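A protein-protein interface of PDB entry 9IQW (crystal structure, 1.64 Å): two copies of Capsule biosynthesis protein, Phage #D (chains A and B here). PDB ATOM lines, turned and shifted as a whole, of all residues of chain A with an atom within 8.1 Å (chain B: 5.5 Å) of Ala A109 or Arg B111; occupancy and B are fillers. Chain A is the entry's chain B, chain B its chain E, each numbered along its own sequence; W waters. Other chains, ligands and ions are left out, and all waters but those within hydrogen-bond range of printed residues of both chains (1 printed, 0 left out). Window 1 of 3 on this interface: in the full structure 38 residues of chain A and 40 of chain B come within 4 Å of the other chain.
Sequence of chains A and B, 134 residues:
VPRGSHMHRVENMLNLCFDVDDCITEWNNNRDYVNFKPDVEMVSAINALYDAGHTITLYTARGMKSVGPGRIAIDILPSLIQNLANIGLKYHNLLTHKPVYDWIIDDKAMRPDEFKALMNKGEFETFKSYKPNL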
ATOM      1  N   CYS A  17      16.973 -21.987   8.533  1.00  0.00           N
ATOM      2  CA  CYS A  17      17.841 -23.123   8.792  1.00  0.00           C
ATOM      3  C   CYS A  17      17.412 -23.824  10.078  1.00  0.00           C
ATOM      4  O   CYS A  17      17.383 -23.201  11.141  1.00  0.00           O
ATOM      5  CB  CYS A  17      19.286 -22.661   8.863  1.00  0.00           C
ATOM      6  SG  CYS A  17      20.471 -24.014   9.039  1.00  0.00           S
ATOM      7  N   TRP A 103      26.512 -23.903  23.127  1.00  0.00           N
ATOM      8  CA  TRP A 103      25.625 -22.803  22.789  1.00  0.00           C
ATOM      9  C   TRP A 103      26.167 -22.014  21.609  1.00  0.00           C
ATOM     10  O   TRP A 103      27.371 -21.767  21.545  1.00  0.00           O
ATOM     11  CB  TRP A 103      25.464 -21.819  23.962  1.00  0.00           C
ATOM     12  CG  TRP A 103      24.683 -22.362  25.112  1.00  0.00           C
ATOM     13  CD1 TRP A 103      25.168 -22.817  26.296  1.00  0.00           C
ATOM     14  CD2 TRP A 103      23.271 -22.542  25.163  1.00  0.00           C
ATOM     15  NE1 TRP A 103      24.141 -23.254  27.090  1.00  0.00           N
ATOM     16  CE2 TRP A 103      22.963 -23.084  26.423  1.00  0.00           C
ATOM     17  CE3 TRP A 103      22.229 -22.262  24.277  1.00  0.00           C
ATOM     18  CZ2 TRP A 103      21.648 -23.374  26.811  1.00  0.00           C
ATOM     19  CZ3 TRP A 103      20.926 -22.540  24.673  1.00  0.00           C
ATOM     20  CH2 TRP A 103      20.654 -23.073  25.927  1.00  0.00           C
ATOM     21  N   ILE A 104      25.250 -21.596  20.729  1.00  0.00           N
ATOM     22  CA  ILE A 104      25.506 -20.539  19.770  1.00  0.00           C
ATOM     23  C   ILE A 104      24.754 -19.306  20.256  1.00  0.00           C
ATOM     24  O   ILE A 104      23.558 -19.389  20.528  1.00  0.00           O
ATOM     25  CB  ILE A 104      25.046 -20.947  18.355  1.00  0.00           C
ATOM     26  CG1 ILE A 104      26.069 -21.901  17.692  1.00  0.00           C
ATOM     27  CG2 ILE A 104      24.784 -19.758  17.473  1.00  0.00           C
ATOM     28  CD1 ILE A 104      25.464 -22.725  16.507  1.00  0.00           C
ATOM     29  N   ILE A 105      25.475 -18.192  20.382  1.00  0.00           N
ATOM     30  CA  ILE A 105      24.895 -16.912  20.728  1.00  0.00           C
ATOM     31  C   ILE A 105      24.905 -16.096  19.445  1.00  0.00           C
ATOM     32  O   ILE A 105      25.959 -15.784  18.908  1.00  0.00           O
ATOM     33  CB  ILE A 105      25.630 -16.229  21.885  1.00  0.00           C
ATOM     34  CG1 ILE A 105      25.643 -17.103  23.148  1.00  0.00           C
ATOM     35  CG2 ILE A 105      24.998 -14.868  22.177  1.00  0.00           C
ATOM     36  CD1 ILE A 105      26.705 -18.153  23.193  1.00  0.00           C
ATOM     37  N   ASP A 106      23.703 -15.764  18.961  1.00  0.00           N
ATOM     38  CA  ASP A 106      23.523 -15.332  17.588  1.00  0.00           C
ATOM     39  C   ASP A 106      22.311 -14.402  17.570  1.00  0.00           C
ATOM     40  O   ASP A 106      21.299 -14.731  18.176  1.00  0.00           O
ATOM     41  CB  ASP A 106      23.327 -16.597  16.722  1.00  0.00           C
ATOM     42  CG  ASP A 106      23.090 -16.428  15.243  1.00  0.00           C
ATOM     43  OD1 ASP A 106      22.462 -15.429  14.854  1.00  0.00           O
ATOM     44  OD2 ASP A 106      23.563 -17.308  14.448  1.00  0.00           O
ATOM     45  N   ASP A 107      22.427 -13.264  16.880  1.00  0.00           N
ATOM     46  CA  ASP A 107      21.347 -12.289  16.821  1.00  0.00           C
ATOM     47  C   ASP A 107      20.089 -12.811  16.127  1.00  0.00           C
ATOM     48  O   ASP A 107      19.010 -12.276  16.354  1.00  0.00           O
ATOM     49  CB  ASP A 107      21.805 -11.006  16.118  1.00  0.00           C
ATOM     50  CG  ASP A 107      22.339 -11.216  14.719  1.00  0.00           C
ATOM     51  OD1 ASP A 107      23.247 -12.083  14.550  1.00  0.00           O
ATOM     52  OD2 ASP A 107      21.882 -10.502  13.793  1.00  0.00           O
ATOM     53  N   LYS A 108      20.245 -13.827  15.278  1.00  0.00           N
ATOM     54  CA  LYS A 108      19.155 -14.383  14.487  1.00  0.00           C
ATOM     55  C   LYS A 108      18.985 -15.871  14.769  1.00  0.00           C
ATOM     56  O   LYS A 108      18.863 -16.683  13.854  1.00  0.00           O
ATOM     57  CB  LYS A 108      19.399 -14.131  12.992  1.00  0.00           C
ATOM     58  CG  LYS A 108      19.289 -12.676  12.620  1.00  0.00           C
ATOM     59  CD  LYS A 108      19.639 -12.372  11.188  1.00  0.00           C
ATOM     60  CE  LYS A 108      19.530 -10.892  10.908  1.00  0.00           C
ATOM     61  NZ  LYS A 108      19.806 -10.583   9.495  1.00  0.00           N
ATOM     62  N   ALA A 109      18.970 -16.210  16.057  1.00  0.00           N
ATOM     63  CA  ALA A 109      18.738 -17.583  16.470  1.00  0.00           C
ATOM     64  C   ALA A 109      17.494 -17.671  17.338  1.00  0.00           C
ATOM     65  O   ALA A 109      17.116 -16.704  17.994  1.00  0.00           O
ATOM     66  CB  ALA A 109      19.916 -18.119  17.209  1.00  0.00           C
ATOM     67  N   MET A 110      16.856 -18.841  17.288  1.00  0.00           N
ATOM     68  CA  MET A 110      15.634 -19.090  18.022  1.00  0.00           C
ATOM     69  C   MET A 110      15.577 -20.586  18.320  1.00  0.00           C
ATOM     70  O   MET A 110      15.988 -21.390  17.488  1.00  0.00           O
ATOM     71  CB  MET A 110      14.502 -18.594  17.109  1.00  0.00           C
ATOM     72  CG  MET A 110      13.172 -19.099  17.409  1.00  0.00           C
ATOM     73  SD  MET A 110      11.927 -18.456  16.268  1.00  0.00           S
ATOM     74  CE  MET A 110      12.439 -16.736  16.042  1.00  0.00           C
ATOM     75  N   ARG A 111      15.097 -20.944  19.512  1.00  0.00           N
ATOM     76  CA  ARG A 111      14.937 -22.347  19.861  1.00  0.00           C
ATOM     77  C   ARG A 111      13.565 -22.828  19.404  1.00  0.00           C
ATOM     78  O   ARG A 111      12.680 -22.018  19.108  1.00  0.00           O
ATOM     79  CB  ARG A 111      15.177 -22.579  21.359  1.00  0.00           C
ATOM     80  CG  ARG A 111      16.595 -22.230  21.796  1.00  0.00           C
ATOM     81  CD  ARG A 111      16.938 -22.725  23.182  1.00  0.00           C
ATOM     82  NE  ARG A 111      16.172 -22.064  24.238  1.00  0.00           N
ATOM     83  CZ  ARG A 111      16.451 -20.879  24.758  1.00  0.00           C
ATOM     84  NH1 ARG A 111      17.485 -20.167  24.342  1.00  0.00           N
ATOM     85  NH2 ARG A 111      15.688 -20.404  25.743  1.00  0.00           N
ATOM     86  N   PRO A 112      13.357 -24.156  19.259  1.00  0.00           N
ATOM     87  CA  PRO A 112      12.110 -24.656  18.681  1.00  0.00           C
ATOM     88  C   PRO A 112      10.849 -24.280  19.455  1.00  0.00           C
ATOM     89  O   PRO A 112       9.777 -24.168  18.855  1.00  0.00           O
ATOM     90  CB  PRO A 112      12.318 -26.170  18.643  1.00  0.00           C
ATOM     91  CG  PRO A 112      13.824 -26.335  18.604  1.00  0.00           C
ATOM     92  CD  PRO A 112      14.349 -25.222  19.492  1.00  0.00           C
ATOM     93  N   GLU A 114      10.237 -21.389  21.054  1.00  0.00           N
ATOM     94  CA  GLU A 114       9.868 -20.046  20.626  1.00  0.00           C
ATOM     95  C   GLU A 114       9.327 -20.044  19.199  1.00  0.00           C
ATOM     96  O   GLU A 114       8.355 -19.353  18.891  1.00  0.00           O
ATOM     97  CB  GLU A 114      11.064 -19.093  20.732  1.00  0.00           C
ATOM     98  CG  GLU A 114      10.682 -17.650  20.454  1.00  0.00           C
ATOM     99  CD  GLU A 114      11.815 -16.651  20.606  1.00  0.00           C
ATOM    100  OE1 GLU A 114      12.999 -17.037  20.474  1.00  0.00           O
ATOM    101  OE2 GLU A 114      11.509 -15.477  20.904  1.00  0.00           O
ATOM    102  N   PHE A 115       9.965 -20.823  18.327  1.00  0.00           N
ATOM    103  CA  PHE A 115       9.515 -20.968  16.955  1.00  0.00           C
ATOM    104  C   PHE A 115       8.069 -21.456  16.902  1.00  0.00           C
ATOM    105  O   PHE A 115       7.232 -20.872  16.203  1.00  0.00           O
ATOM    106  CB  PHE A 115      10.434 -21.930  16.202  1.00  0.00           C
ATOM    107  CG  PHE A 115       9.915 -22.301  14.834  1.00  0.00           C
ATOM    108  CD1 PHE A 115       9.969 -21.402  13.790  1.00  0.00           C
ATOM    109  CD2 PHE A 115       9.331 -23.540  14.607  1.00  0.00           C
ATOM    110  CE1 PHE A 115       9.497 -21.744  12.532  1.00  0.00           C
ATOM    111  CE2 PHE A 115       8.858 -23.877  13.349  1.00  0.00           C
ATOM    112  CZ  PHE A 115       8.937 -22.976  12.320  1.00  0.00           C
ATOM    113  N   LEU A 118       5.599 -18.713  18.239  1.00  0.00           N
ATOM    114  CA  LEU A 118       5.376 -17.652  17.274  1.00  0.00           C
ATOM    115  C   LEU A 118       4.517 -18.144  16.113  1.00  0.00           C
ATOM    116  O   LEU A 118       3.628 -17.428  15.666  1.00  0.00           O
ATOM    117  CB  LEU A 118       6.712 -17.108  16.772  1.00  0.00           C
ATOM    118  CG  LEU A 118       7.528 -16.307  17.786  1.00  0.00           C
ATOM    119  CD1 LEU A 118       8.961 -16.106  17.286  1.00  0.00           C
ATOM    120  CD2 LEU A 118       6.881 -14.982  18.079  1.00  0.00           C
ATOM    121  N   PHE A 127       8.554 -11.388  13.114  1.00  0.00           N
ATOM    122  CA  PHE A 127       9.279 -11.286  14.370  1.00  0.00           C
ATOM    123  C   PHE A 127      10.657 -10.687  14.097  1.00  0.00           C
ATOM    124  O   PHE A 127      11.336 -11.101  13.161  1.00  0.00           O
ATOM    125  CB  PHE A 127       9.405 -12.663  15.029  1.00  0.00           C
ATOM    126  CG  PHE A 127       9.991 -12.634  16.420  1.00  0.00           C
ATOM    127  CD1 PHE A 127       9.283 -12.107  17.476  1.00  0.00           C
ATOM    128  CD2 PHE A 127      11.248 -13.165  16.672  1.00  0.00           C
ATOM    129  CE1 PHE A 127       9.806 -12.103  18.755  1.00  0.00           C
ATOM    130  CE2 PHE A 127      11.776 -13.155  17.950  1.00  0.00           C
ATOM    131  CZ  PHE A 127      11.051 -12.613  18.990  1.00  0.00           C
ATOM    132  N   LYS A 128      11.058  -9.717  14.927  1.00  0.00           N
ATOM    133  CA  LYS A 128      12.307  -9.001  14.713  1.00  0.00           C
ATOM    134  C   LYS A 128      13.458  -9.686  15.443  1.00  0.00           C
ATOM    135  O   LYS A 128      13.321 -10.082  16.594  1.00  0.00           O
ATOM    136  CB  LYS A 128      12.181  -7.542  15.189  1.00  0.00           C
ATOM    137  CG  LYS A 128      11.240  -6.709  14.319  1.00  0.00           C
ATOM    138  CD  LYS A 128      10.914  -5.340  14.938  1.00  0.00           C
ATOM    139  CE  LYS A 128      10.117  -4.438  14.011  1.00  0.00           C
ATOM    140  NZ  LYS A 128      10.201  -4.889  12.596  1.00  0.00           N
ATOM    141  N   SER A 129      14.596  -9.789  14.760  1.00  0.00           N
ATOM    142  CA  SER A 129      15.811 -10.296  15.368  1.00  0.00           C
ATOM    143  C   SER A 129      16.452  -9.269  16.299  1.00  0.00           C
ATOM    144  O   SER A 129      16.042  -8.109  16.362  1.00  0.00           O
ATOM    145  CB  SER A 129      16.776 -10.752  14.280  1.00  0.00           C
ATOM    146  OG  SER A 129      17.125  -9.706  13.409  1.00  0.00           O
ATOM    147  N   TYR A 130      17.459  -9.720  17.052  1.00  0.00           N
ATOM    148  CA  TYR A 130      18.098  -8.890  18.055  1.00  0.00           C
ATOM    149  C   TYR A 130      18.989  -7.808  17.453  1.00  0.00           C
ATOM    150  O   TYR A 130      19.721  -8.063  16.487  1.00  0.00           O
ATOM    151  CB  TYR A 130      18.940  -9.774  18.978  1.00  0.00           C
ATOM    152  CG  TYR A 130      19.833  -9.005  19.917  1.00  0.00           C
ATOM    153  CD1 TYR A 130      19.383  -8.604  21.163  1.00  0.00           C
ATOM    154  CD2 TYR A 130      21.127  -8.664  19.554  1.00  0.00           C
ATOM    155  CE1 TYR A 130      20.195  -7.884  22.026  1.00  0.00           C
ATOM    156  CE2 TYR A 130      21.951  -7.945  20.411  1.00  0.00           C
ATOM    157  CZ  TYR A 130      21.491  -7.579  21.659  1.00  0.00           C
ATOM    158  OH  TYR A 130      22.266  -6.860  22.531  1.00  0.00           O
ATOM    159  N   LYS A 131      18.929  -6.616  18.048  1.00  0.00           N
ATOM    160  CA  LYS A 131      19.857  -5.536  17.741  1.00  0.00           C
ATOM    161  C   LYS A 131      20.402  -4.975  19.052  1.00  0.00           C
ATOM    162  O   LYS A 131      19.659  -4.853  20.032  1.00  0.00           O
ATOM    163  CB  LYS A 131      19.170  -4.397  16.958  1.00  0.00           C
ATOM    164  CG  LYS A 131      18.503  -4.826  15.653  1.00  0.00           C
ATOM    165  CD  LYS A 131      19.471  -5.293  14.585  1.00  0.00           C
ATOM    166  CE  LYS A 131      18.750  -5.696  13.319  1.00  0.00           C
ATOM    167  NZ  LYS A 131      19.649  -6.385  12.374  1.00  0.00           N
ATOM    168  N   TRP B 103      16.919 -16.825   9.984  1.00  0.00           N
ATOM    169  CA  TRP B 103      16.812 -17.472  11.275  1.00  0.00           C
ATOM    170  C   TRP B 103      17.487 -18.840  11.243  1.00  0.00           C
ATOM    171  O   TRP B 103      17.340 -19.569  10.266  1.00  0.00           O
ATOM    172  CB  TRP B 103      15.353 -17.708  11.700  1.00  0.00           C
ATOM    173  CG  TRP B 103      14.601 -16.460  12.013  1.00  0.00           C
ATOM    174  CD1 TRP B 103      13.683 -15.834  11.233  1.00  0.00           C
ATOM    175  CD2 TRP B 103      14.738 -15.666  13.196  1.00  0.00           C
ATOM    176  NE1 TRP B 103      13.216 -14.705  11.870  1.00  0.00           N
ATOM    177  CE2 TRP B 103      13.859 -14.573  13.069  1.00  0.00           C
ATOM    178  CE3 TRP B 103      15.497 -15.787  14.355  1.00  0.00           C
ATOM    179  CZ2 TRP B 103      13.741 -13.594  14.059  1.00  0.00           C
ATOM    180  CZ3 TRP B 103      15.366 -14.818  15.340  1.00  0.00           C
ATOM    181  CH2 TRP B 103      14.509 -13.732  15.172  1.00  0.00           C
ATOM    182  N   ILE B 104      18.209 -19.145  12.326  1.00  0.00           N
ATOM    183  CA  ILE B 104      18.554 -20.512  12.666  1.00  0.00           C
ATOM    184  C   ILE B 104      17.651 -20.955  13.807  1.00  0.00           C
ATOM    185  O   ILE B 104      17.566 -20.270  14.819  1.00  0.00           O
ATOM    186  CB  ILE B 104      20.046 -20.699  13.029  1.00  0.00           C
ATOM    187  CG1 ILE B 104      20.492 -19.836  14.182  1.00  0.00           C
ATOM    188  CG2 ILE B 104      20.915 -20.469  11.806  1.00  0.00           C
ATOM    189  CD1 ILE B 104      21.725 -20.399  14.947  1.00  0.00           C
ATOM    190  N   ALA B 109      20.632 -22.683  20.829  1.00  0.00           N
ATOM    191  CA  ALA B 109      20.876 -21.315  20.404  1.00  0.00           C
ATOM    192  C   ALA B 109      20.208 -20.330  21.351  1.00  0.00           C
ATOM    193  O   ALA B 109      19.230 -20.664  22.012  1.00  0.00           O
ATOM    194  CB  ALA B 109      20.391 -21.102  19.009  1.00  0.00           C
ATOM    195  N   MET B 110      20.750 -19.113  21.401  1.00  0.00           N
ATOM    196  CA  MET B 110      20.304 -18.085  22.320  1.00  0.00           C
ATOM    197  C   MET B 110      20.675 -16.738  21.704  1.00  0.00           C
ATOM    198  O   MET B 110      21.718 -16.613  21.069  1.00  0.00           O
ATOM    199  CB  MET B 110      21.006 -18.362  23.659  1.00  0.00           C
ATOM    200  CG  MET B 110      21.115 -17.243  24.571  1.00  0.00           C
ATOM    201  SD  MET B 110      21.905 -17.690  26.117  1.00  0.00           S
ATOM    202  CE  MET B 110      21.173 -19.299  26.533  1.00  0.00           C
ATOM    203  N   ARG B 111      19.806 -15.733  21.848  1.00  0.00           N
ATOM    204  CA  ARG B 111      20.123 -14.400  21.381  1.00  0.00           C
ATOM    205  C   ARG B 111      20.857 -13.631  22.477  1.00  0.00           C
ATOM    206  O   ARG B 111      20.827 -14.009  23.647  1.00  0.00           O
ATOM    207  CB  ARG B 111      18.853 -13.665  20.889  1.00  0.00           C
ATOM    208  CG  ARG B 111      18.185 -14.364  19.719  1.00  0.00           C
ATOM    209  CD  ARG B 111      17.117 -13.511  19.044  1.00  0.00           C
ATOM    210  NE  ARG B 111      15.959 -13.310  19.913  1.00  0.00           N
ATOM    211  CZ  ARG B 111      14.963 -14.176  20.066  1.00  0.00           C
ATOM    212  NH1 ARG B 111      14.961 -15.348  19.453  1.00  0.00           N
ATOM    213  NH2 ARG B 111      13.950 -13.870  20.872  1.00  0.00           N
ATOM    214  N   PRO B 112      21.585 -12.550  22.130  1.00  0.00           N
ATOM    215  CA  PRO B 112      22.412 -11.852  23.104  1.00  0.00           C
ATOM    216  C   PRO B 112      21.662 -11.275  24.302  1.00  0.00           C
ATOM    217  O   PRO B 112      22.236 -11.162  25.381  1.00  0.00           O
ATOM    218  CB  PRO B 112      23.095 -10.773  22.265  1.00  0.00           C
ATOM    219  CG  PRO B 112      23.138 -11.335  20.881  1.00  0.00           C
ATOM    220  CD  PRO B 112      21.796 -12.053  20.757  1.00  0.00           C
ATOM    221  N   ASP B 113      20.401 -10.876  24.098  1.00  0.00           N
ATOM    222  CA  ASP B 113      19.615 -10.351  25.202  1.00  0.00           C
ATOM    223  C   ASP B 113      19.400 -11.407  26.285  1.00  0.00           C
ATOM    224  O   ASP B 113      19.569 -11.119  27.470  1.00  0.00           O
ATOM    225  CB  ASP B 113      18.289  -9.732  24.729  1.00  0.00           C
ATOM    226  CG  ASP B 113      17.413 -10.529  23.785  1.00  0.00           C
ATOM    227  OD1 ASP B 113      17.805 -11.676  23.413  1.00  0.00           O
ATOM    228  OD2 ASP B 113      16.375  -9.989  23.362  1.00  0.00           O
ATOM    229  N   GLU B 114      19.020 -12.621  25.881  1.00  0.00           N
ATOM    230  CA  GLU B 114      18.842 -13.711  26.836  1.00  0.00           C
ATOM    231  C   GLU B 114      20.168 -14.097  27.492  1.00  0.00           C
ATOM    232  O   GLU B 114      20.228 -14.359  28.694  1.00  0.00           O
ATOM    233  CB  GLU B 114      18.240 -14.941  26.158  1.00  0.00           C
ATOM    234  CG  GLU B 114      17.904 -16.067  27.118  1.00  0.00           C
ATOM    235  CD  GLU B 114      17.229 -17.255  26.453  1.00  0.00           C
ATOM    236  OE1 GLU B 114      17.398 -17.448  25.227  1.00  0.00           O
ATOM    237  OE2 GLU B 114      16.529 -17.997  27.172  1.00  0.00           O
ATOM    238  N   PHE B 115      21.230 -14.126  26.685  1.00  0.00           N
ATOM    239  CA  PHE B 115      22.566 -14.408  27.186  1.00  0.00           C
ATOM    240  C   PHE B 115      22.943 -13.429  28.300  1.00  0.00           C
ATOM    241  O   PHE B 115      23.379 -13.834  29.370  1.00  0.00           O
ATOM    242  CB  PHE B 115      23.572 -14.357  26.048  1.00  0.00           C
ATOM    243  CG  PHE B 115      25.000 -14.426  26.516  1.00  0.00           C
ATOM    244  CD1 PHE B 115      25.542 -15.622  26.946  1.00  0.00           C
ATOM    245  CD2 PHE B 115      25.798 -13.291  26.531  1.00  0.00           C
ATOM    246  CE1 PHE B 115      26.854 -15.690  27.384  1.00  0.00           C
ATOM    247  CE2 PHE B 115      27.118 -13.359  26.956  1.00  0.00           C
ATOM    248  CZ  PHE B 115      27.644 -14.556  27.392  1.00  0.00           C
ATOM    249  N   LYS B 116      22.763 -12.132  28.039  1.00  0.00           N
ATOM    250  CA  LYS B 116      23.091 -11.121  29.031  1.00  0.00           C
ATOM    251  C   LYS B 116      22.239 -11.250  30.295  1.00  0.00           C
ATOM    252  O   LYS B 116      22.742 -11.068  31.406  1.00  0.00           O
ATOM    253  CB  LYS B 116      22.964  -9.726  28.422  1.00  0.00           C
ATOM    254  CG  LYS B 116      24.120  -9.388  27.511  1.00  0.00           C
ATOM    255  CD  LYS B 116      24.048  -7.955  26.967  1.00  0.00           C
ATOM    256  CE  LYS B 116      23.054  -7.807  25.865  1.00  0.00           C
ATOM    257  NZ  LYS B 116      22.891  -6.377  25.498  1.00  0.00           N
HETATM  258  O   HOH W   1      10.916 -12.973  11.276  1.00  0.00           O
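The backbone carbonyl oxygen of Trp B103 is in hydrogen-bond range of the backbone NH of Cys A17.
The backbone NH of Met B110 sits at hydrogen-bond distance from the backbone carbonyl oxygen of Ile A104 (3.0 Å).
The backbone NH (N) of Asp A106 sits at hydrogen-bond distance from the backbone carbonyl oxygen (O) of Met B110, at 3.0 Å.
The backbone carbonyl oxygen (O) of Lys A108 lies within hydrogen-bond range of the backbone NH (N) of Ile B104 (3.0 Å).
NH1 of Arg B111 is in hydrogen-bond range of O of Ala A109 (2.9 Å).
The backbone NH (N) of Met A110 sits at hydrogen-bond distance from the backbone carbonyl oxygen (O) of Ile B104.
The backbone carbonyl oxygen (O) of Ala B109 sits at hydrogen-bond distance from the guanidinium group (NH1) of Arg A111 (3.0 Å).
NH1 of Arg A111 lies within salt-bridge range of OE1 of Glu B114 (2.9 Å).
OE1 of Glu A114 is in salt-bridge range of NH1 of Arg B111 (2.8 Å).
The side-chain hydroxyl (OH) of Tyr A130 is in hydrogen-bond range of the side-chain amino group (NZ) of Lys B116, at 3.1 Å.
The side-chain carboxylate of Asp A106 lies within hydrogen-bond range of the backbone NH of Lys A108 (2.8 Å).
The backbone NH (N) of Tyr A130 sits at hydrogen-bond distance from the backbone carbonyl oxygen (O) of Asp A107 (3.1 Å).
The side-chain sulfur of Met A110 lies close to the backbone NH of Phe A115 (3.7 Å).
The side-chain sulfur (SD) of Met B110 lies close to the backbone NH (N) of Phe B115 (3.7 Å).
Among the printed residues, merely in contact across the chains: Cys A17 with Ile B104 (3.3 Å), Trp A103 with Ala B109 (3.7 Å), Trp A103 with Met B110 (3.7 Å), Ile A104 with Ala B109 (3.3 Å), Ile A105 with Met B110 (3.2 Å), Asp A106 with Ile B104 (3.6 Å), Asp A106 with Arg B111 (3.4 Å), Asp A106 with Pro B112 (3.8 Å), Asp A107 with Arg B111 (3.5 Å), Asp A107 with Pro B112 (3.97 Å), Lys A108 with Trp B103 (3.4 Å), Ala A109 with Trp B103 (3.7 Å), Ala A109 with Ile B104 (3.4 Å), Ala A109 with Ala B109 (3.5 Å), Met A110 with Trp B103 (3.6 Å), Phe A127 with Trp B103 (3.6 Å), Phe A127 with Arg B111 (3.7 Å), Ser A129 with Trp B103 (3.7 Å), Tyr A130 with Pro B112 (3.6 Å) and Tyr A130 with Asp B113 (3.6 Å).
Ala A109 touches four residues of chain B.
Of chain A, only Asp A106, Asp A107, Ala A109, Glu A114 and Phe A127 come within 4 Å of Arg B111.
Pro B112 touches just these residues of chain A: Asp A106, Asp A107 and Tyr A130.
Of the printed residues of chain B, Asp A106 touches Ile B104 (3.6 Å), Met B110 (3.0 Å), Arg B111 (3.4 Å) and Pro B112 (3.8 Å).
Printed residues of chain B within 4 Å of Phe A127: Trp B103 and Arg B111.
Phe A115 touches none of the printed residues of chain B.
The nearest residue of chain B that does not touch Ala A109 is Met B110 (4.4 Å).
The nearest printed residue of chain A that does not touch Glu B114 is Tyr A130 (6.2 Å).
Of the 19 printed residues of chain A, 14 touch a printed residue of chain B.
Printed residues of chain A that touch a printed residue of chain B: Cys A17, Trp A103, Ile A104, Ile A105, Asp A106, Asp A107, Lys A108, Ala A109, Met A110, Arg A111, Glu A114, Phe A127, Ser A129 and Tyr A130.
Hydrophobic or aromatic side chains of chain A that line the printed part of chain B: Trp A103, Ile A105, Ala A109, Met A110, Phe A127 and Tyr A130.
Hydrophobic or aromatic side chains of chain B that line the printed part of chain A: Trp B103, Ile B104, Ala B109, Met B110 and Pro B112.
Among the printed residues, 30 pairs touch across the chains.
Among the printed residues, Asp or Glu carboxylates within 4 Å of a Lys or Arg side-chain nitrogen of the other chain: Arg A111 with Glu B114 and Glu A114 with Arg B111.
Ile A104 touches Ala B109, and with the chains exchanged Ala A109 touches Ile B104.
Ile A104 touches Met B110, and with the chains exchanged Met A110 touches Ile B104.
Ala A109 touches its own counterpart, Ala B109.
Ala A109 touches Arg B111, and with the chains exchanged Arg A111 touches Ala B109.
Water W1 lies within hydrogen-bond range of the backbone carbonyl oxygen of Phe A127 (2.7 Å) and the indole nitrogen of Trp B103 (2.9 Å).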
